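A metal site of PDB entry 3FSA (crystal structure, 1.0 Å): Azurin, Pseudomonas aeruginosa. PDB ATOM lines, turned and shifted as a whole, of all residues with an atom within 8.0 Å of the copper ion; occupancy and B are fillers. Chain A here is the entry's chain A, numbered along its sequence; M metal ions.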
ATOM      1  N   GLY A   9      27.519   3.850  15.093  1.00  0.00           N
ATOM      2  CA  GLY A   9      26.075   3.677  15.118  1.00  0.00           C
ATOM      3  C   GLY A   9      25.693   2.753  13.962  1.00  0.00           C
ATOM      4  O   GLY A   9      26.119   2.991  12.835  1.00  0.00           O
ATOM      5  N   ASN A  10      24.929   1.693  14.235  1.00  0.00           N
ATOM      6  CA  ASN A  10      24.754   0.635  13.257  1.00  0.00           C
ATOM      7  C   ASN A  10      23.338   0.519  12.718  1.00  0.00           C
ATOM      8  O   ASN A  10      22.459   1.353  12.972  1.00  0.00           O
ATOM      9  CB  ASN A  10      25.295  -0.689  13.798  1.00  0.00           C
ATOM     10  CG  ASN A  10      24.459  -1.264  14.868  1.00  0.00           C
ATOM     11  OD1 ASN A  10      23.391  -0.744  15.186  1.00  0.00           O
ATOM     12  ND2 ASN A  10      24.937  -2.382  15.466  1.00  0.00           N
ATOM     13  N   MET A  13      20.152   0.444  15.121  1.00  0.00           N
ATOM     14  CA  MET A  13      19.701   1.624  15.876  1.00  0.00           C
ATOM     15  C   MET A  13      20.335   1.629  17.262  1.00  0.00           C
ATOM     16  O   MET A  13      19.680   1.928  18.269  1.00  0.00           O
ATOM     17  CB  MET A  13      18.157   1.749  15.927  1.00  0.00           C
ATOM     18  CG  MET A  13      17.650   3.178  16.255  1.00  0.00           C
ATOM     19  SD  MET A  13      15.914   3.258  16.629  1.00  0.00           S
ATOM     20  CE  MET A  13      15.890   2.583  18.289  1.00  0.00           C
ATOM     21  N   GLN A  14      21.656   1.375  17.308  1.00  0.00           N
ATOM     22  CA  GLN A  14      22.383   1.444  18.531  1.00  0.00           C
ATOM     23  C   GLN A  14      23.829   1.965  18.290  1.00  0.00           C
ATOM     24  O   GLN A  14      24.457   1.684  17.255  1.00  0.00           O
ATOM     25  CB  GLN A  14      22.176   0.125  19.351  1.00  0.00           C
ATOM     26  CG  GLN A  14      23.044  -1.015  18.838  1.00  0.00           C
ATOM     27  N   PHE A  15      24.308   2.729  19.284  1.00  0.00           N
ATOM     28  CA  PHE A  15      25.704   3.038  19.387  1.00  0.00           C
ATOM     29  C   PHE A  15      26.406   1.858  20.050  1.00  0.00           C
ATOM     30  O   PHE A  15      25.777   1.038  20.730  1.00  0.00           O
ATOM     31  CB  PHE A  15      25.948   4.288  20.278  1.00  0.00           C
ATOM     32  CG  PHE A  15      25.493   5.602  19.707  1.00  0.00           C
ATOM     33  CD1 PHE A  15      25.989   6.082  18.504  1.00  0.00           C
ATOM     34  CD2 PHE A  15      24.622   6.414  20.428  1.00  0.00           C
ATOM     35  CE1 PHE A  15      25.619   7.352  18.038  1.00  0.00           C
ATOM     36  CE2 PHE A  15      24.263   7.661  19.963  1.00  0.00           C
ATOM     37  CZ  PHE A  15      24.775   8.140  18.750  1.00  0.00           C
ATOM     38  N   LEU A  33      32.763   9.465  14.575  1.00  0.00           N
ATOM     39  CA  LEU A  33      31.559   8.656  14.395  1.00  0.00           C
ATOM     40  C   LEU A  33      31.640   7.924  13.043  1.00  0.00           C
ATOM     41  O   LEU A  33      31.989   8.501  12.009  1.00  0.00           O
ATOM     42  CB  LEU A  33      30.335   9.559  14.411  1.00  0.00           C
ATOM     43  CG  LEU A  33      28.992   8.848  14.277  1.00  0.00           C
ATOM     44  CD1 LEU A  33      28.644   7.977  15.488  1.00  0.00           C
ATOM     45  CD2 LEU A  33      27.868   9.859  14.004  1.00  0.00           C
ATOM     46  N   HIS A  35      29.524   4.433  10.755  1.00  0.00           N
ATOM     47  CA  HIS A  35      28.253   3.720  10.623  1.00  0.00           C
ATOM     48  C   HIS A  35      28.519   2.385   9.879  1.00  0.00           C
ATOM     49  O   HIS A  35      28.292   2.265   8.685  1.00  0.00           O
ATOM     50  CB  HIS A  35      27.248   4.565   9.828  1.00  0.00           C
ATOM     51  CG  HIS A  35      25.850   4.036   9.788  1.00  0.00           C
ATOM     52  ND1 HIS A  35      25.491   2.703   9.651  1.00  0.00           N
ATOM     53  CD2 HIS A  35      24.688   4.729   9.782  1.00  0.00           C
ATOM     54  CE1 HIS A  35      24.172   2.612   9.581  1.00  0.00           C
ATOM     55  NE2 HIS A  35      23.661   3.825   9.653  1.00  0.00           N
ATOM     56  N   MET A  44      18.390   4.868   7.862  1.00  0.00           N
ATOM     57  CA  MET A  44      18.922   4.656   9.230  1.00  0.00           C
ATOM     58  C   MET A  44      20.157   5.553   9.409  1.00  0.00           C
ATOM     59  O   MET A  44      21.239   5.050   9.752  1.00  0.00           O
ATOM     60  CB  MET A  44      19.291   3.168   9.462  1.00  0.00           C
ATOM     61  CG  MET A  44      19.555   2.753  10.940  1.00  0.00           C
ATOM     62  SD  MET A  44      18.263   3.161  12.144  1.00  0.00           S
ATOM     63  CE  MET A  44      16.999   1.979  11.639  1.00  0.00           C
ATOM     64  N   GLY A  45      20.050   6.848   9.168  1.00  0.00           N
ATOM     65  CA  GLY A  45      21.129   7.769   9.435  1.00  0.00           C
ATOM     66  C   GLY A  45      21.228   8.081  10.925  1.00  0.00           C
ATOM     67  O   GLY A  45      20.222   8.110  11.639  1.00  0.00           O
ATOM     68  N   HIS A  46      22.470   8.314  11.380  1.00  0.00           N
ATOM     69  CA  HIS A  46      22.742   8.672  12.762  1.00  0.00           C
ATOM     70  C   HIS A  46      23.575   9.938  12.833  1.00  0.00           C
ATOM     71  O   HIS A  46      24.408  10.177  11.958  1.00  0.00           O
ATOM     72  CB  HIS A  46      23.516   7.590  13.543  1.00  0.00           C
ATOM     73  CG  HIS A  46      22.850   6.251  13.521  1.00  0.00           C
ATOM     74  ND1 HIS A  46      21.569   6.073  14.016  1.00  0.00           N
ATOM     75  CD2 HIS A  46      23.321   5.054  13.084  1.00  0.00           C
ATOM     76  CE1 HIS A  46      21.303   4.787  13.868  1.00  0.00           C
ATOM     77  NE2 HIS A  46      22.323   4.138  13.303  1.00  0.00           N
ATOM     78  N   ASN A  47      23.420  10.690  13.914  1.00  0.00           N
ATOM     79  CA  ASN A  47      24.395  11.698  14.286  1.00  0.00           C
ATOM     80  C   ASN A  47      24.773  11.467  15.768  1.00  0.00           C
ATOM     81  O   ASN A  47      24.323  10.532  16.410  1.00  0.00           O
ATOM     82  CB  ASN A  47      23.926  13.120  13.959  1.00  0.00           C
ATOM     83  CG  ASN A  47      22.750  13.593  14.773  1.00  0.00           C
ATOM     84  OD1 ASN A  47      22.271  12.880  15.657  1.00  0.00           O
ATOM     85  ND2 ASN A  47      22.258  14.784  14.461  1.00  0.00           N
ATOM     86  N   TRP A  48      25.629  12.360  16.249  1.00  0.00           N
ATOM     87  CA  TRP A  48      26.096  12.308  17.642  1.00  0.00           C
ATOM     88  C   TRP A  48      25.993  13.734  18.162  1.00  0.00           C
ATOM     89  O   TRP A  48      26.545  14.673  17.531  1.00  0.00           O
ATOM     90  CB  TRP A  48      27.506  11.754  17.703  1.00  0.00           C
ATOM     91  CG  TRP A  48      28.085  11.624  19.095  1.00  0.00           C
ATOM     92  CD1 TRP A  48      28.097  10.482  19.842  1.00  0.00           C
ATOM     93  CD2 TRP A  48      28.745  12.627  19.872  1.00  0.00           C
ATOM     94  NE1 TRP A  48      28.747  10.699  21.035  1.00  0.00           N
ATOM     95  CE2 TRP A  48      29.148  12.004  21.092  1.00  0.00           C
ATOM     96  CE3 TRP A  48      29.081  13.983  19.648  1.00  0.00           C
ATOM     97  CZ2 TRP A  48      29.797  12.709  22.101  1.00  0.00           C
ATOM     98  CZ3 TRP A  48      29.762  14.663  20.655  1.00  0.00           C
ATOM     99  CH2 TRP A  48      30.104  14.029  21.875  1.00  0.00           C
ATOM    100  N   LEU A  86      24.705  14.051  10.071  1.00  0.00           N
ATOM    101  CA  LEU A  86      23.992  12.784   9.926  1.00  0.00           C
ATOM    102  C   LEU A  86      24.716  11.928   8.882  1.00  0.00           C
ATOM    103  O   LEU A  86      25.029  12.407   7.766  1.00  0.00           O
ATOM    104  CB  LEU A  86      22.581  13.051   9.415  1.00  0.00           C
ATOM    105  CG  LEU A  86      21.653  11.833   9.411  1.00  0.00           C
ATOM    106  CD1 LEU A  86      21.124  11.612  10.806  1.00  0.00           C
ATOM    107  CD2 LEU A  86      20.519  12.004   8.449  1.00  0.00           C
ATOM    108  N   ILE A  87      25.000  10.673   9.248  1.00  0.00           N
ATOM    109  CA  ILE A  87      25.733   9.756   8.376  1.00  0.00           C
ATOM    110  C   ILE A  87      24.929   8.470   8.164  1.00  0.00           C
ATOM    111  O   ILE A  87      24.241   7.972   9.064  1.00  0.00           O
ATOM    112  CB  ILE A  87      27.155   9.423   8.915  1.00  0.00           C
ATOM    113  CG1 ILE A  87      27.139   8.729  10.270  1.00  0.00           C
ATOM    114  CG2 ILE A  87      28.006  10.692   8.941  1.00  0.00           C
ATOM    115  CD1 ILE A  87      28.466   8.151  10.674  1.00  0.00           C
ATOM    116  N   PHE A 111      23.711  11.608  22.390  1.00  0.00           N
ATOM    117  CA  PHE A 111      22.561  10.934  21.824  1.00  0.00           C
ATOM    118  C   PHE A 111      22.536  11.172  20.318  1.00  0.00           C
ATOM    119  O   PHE A 111      23.213  12.049  19.800  1.00  0.00           O
ATOM    120  CB  PHE A 111      21.231  11.386  22.490  1.00  0.00           C
ATOM    121  CG  PHE A 111      21.024  12.866  22.479  1.00  0.00           C
ATOM    122  CD1 PHE A 111      20.236  13.453  21.498  1.00  0.00           C
ATOM    123  CD2 PHE A 111      21.624  13.676  23.432  1.00  0.00           C
ATOM    124  CE1 PHE A 111      20.049  14.847  21.493  1.00  0.00           C
ATOM    125  CE2 PHE A 111      21.412  15.054  23.427  1.00  0.00           C
ATOM    126  CZ  PHE A 111      20.653  15.614  22.459  1.00  0.00           C
ATOM    127  N   CYS A 112      21.740  10.353  19.638  1.00  0.00           N
ATOM    128  CA  CYS A 112      21.417  10.568  18.226  1.00  0.00           C
ATOM    129  C   CYS A 112      20.111  11.351  18.148  1.00  0.00           C
ATOM    130  O   CYS A 112      19.119  10.990  18.787  1.00  0.00           O
ATOM    131  CB  CYS A 112      21.232   9.197  17.523  1.00  0.00           C
ATOM    132  SG  CYS A 112      20.741   9.399  15.808  1.00  0.00           S
ATOM    133  N   ALA A 113      20.122  12.459  17.405  1.00  0.00           N
ATOM    134  CA  ALA A 113      18.886  13.246  17.286  1.00  0.00           C
ATOM    135  C   ALA A 113      17.842  12.531  16.385  1.00  0.00           C
ATOM    136  O   ALA A 113      16.642  12.818  16.509  1.00  0.00           O
ATOM    137  CB  ALA A 113      19.183  14.628  16.697  1.00  0.00           C
ATOM    138  N   ALA A 114      18.265  11.678  15.465  1.00  0.00           N
ATOM    139  CA  ALA A 114      17.302  10.919  14.661  1.00  0.00           C
ATOM    140  C   ALA A 114      16.586   9.880  15.516  1.00  0.00           C
ATOM    141  O   ALA A 114      15.411   9.580  15.291  1.00  0.00           O
ATOM    142  CB  ALA A 114      17.937  10.236  13.468  1.00  0.00           C
ATOM    143  N   HIS A 115      17.329   9.265  16.447  1.00  0.00           N
ATOM    144  CA  HIS A 115      16.857   8.170  17.283  1.00  0.00           C
ATOM    145  C   HIS A 115      17.250   8.482  18.713  1.00  0.00           C
ATOM    146  O   HIS A 115      18.284   7.981  19.204  1.00  0.00           O
ATOM    147  CB  HIS A 115      17.476   6.838  16.836  1.00  0.00           C
ATOM    148  CG  HIS A 115      17.392   6.612  15.378  1.00  0.00           C
ATOM    149  ND1 HIS A 115      18.533   6.693  14.580  1.00  0.00           N
ATOM    150  CD2 HIS A 115      16.330   6.327  14.576  1.00  0.00           C
ATOM    151  CE1 HIS A 115      18.126   6.463  13.343  1.00  0.00           C
ATOM    152  NE2 HIS A 115      16.820   6.254  13.311  1.00  0.00           N
ATOM    153  N   ALA A 116      16.438   9.258  19.403  1.00  0.00           N
ATOM    154  CA  ALA A 116      16.815   9.770  20.704  1.00  0.00           C
ATOM    155  C   ALA A 116      16.949   8.687  21.768  1.00  0.00           C
ATOM    156  O   ALA A 116      17.526   8.917  22.843  1.00  0.00           O
ATOM    157  CB  ALA A 116      15.834  10.875  21.135  1.00  0.00           C
ATOM    158  N   ALA A 117      16.410   7.506  21.511  1.00  0.00           N
ATOM    159  CA  ALA A 117      16.657   6.365  22.387  1.00  0.00           C
ATOM    160  C   ALA A 117      18.111   5.939  22.424  1.00  0.00           C
ATOM    161  O   ALA A 117      18.522   5.271  23.380  1.00  0.00           O
ATOM    162  CB  ALA A 117      15.807   5.160  21.958  1.00  0.00           C
ATOM    163  N   MET A 118      18.895   6.264  21.382  1.00  0.00           N
ATOM    164  CA  MET A 118      20.326   5.976  21.307  1.00  0.00           C
ATOM    165  C   MET A 118      21.063   7.045  22.121  1.00  0.00           C
ATOM    166  O   MET A 118      21.078   8.214  21.733  1.00  0.00           O
ATOM    167  CB  MET A 118      20.855   6.081  19.852  1.00  0.00           C
ATOM    168  CG  MET A 118      20.272   5.019  18.944  1.00  0.00           C
ATOM    169  SD  MET A 118      20.749   5.245  17.201  1.00  0.00           S
ATOM    170  CE  MET A 118      22.524   5.285  17.268  1.00  0.00           C
HETATM  171 CU    CU M   1      20.375   7.361  15.043  1.00  0.00          CU
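N of Cys 112 sits at hydrogen-bond distance from O of Met 118 (3.1 Å).
O of Asn 10 lies within hydrogen-bond range of NE2 of His 46, at 2.8 Å.
The side-chain sulfur of Cys 112 lies close to the backbone NH of Asn 47, at 3.5 Å.
N of Ala 114 sits close to SG of Cys 112.
SD of Met 44 lies close to NE2 of His 115, 3.6 Å away.
The backbone carbonyl oxygen (O) of His 46 sits at hydrogen-bond distance from the backbone NH (N) of Ile 87 (2.8 Å).
ND1 of His 115 lies close to SD of Met 118 (3.7 Å).
A ring nitrogen (ND1) of His 46 sits close to the side-chain sulfur (SD) of Met 118 (3.4 Å).
O of Gly 45 touches the copper ion, at 3.5 Å.
Five residues have an atom within 4 Å of the copper ion: Gly 45, His 46, Cys 112, His 115 and Met 118.
The nearest printed residue that does not touch the copper ion is Ala 114 (4.1 Å).
The copper ion is bound by a ring nitrogen (ND1) of His 115 (2.0 Å), a ring nitrogen (ND1) of His 46 (2.0 Å) and the side-chain sulfur (SG) of Cys 112 (2.2 Å).
Slightly farther from the copper ion lies the side-chain sulfur (SD) of Met 118 (3.0 Å).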
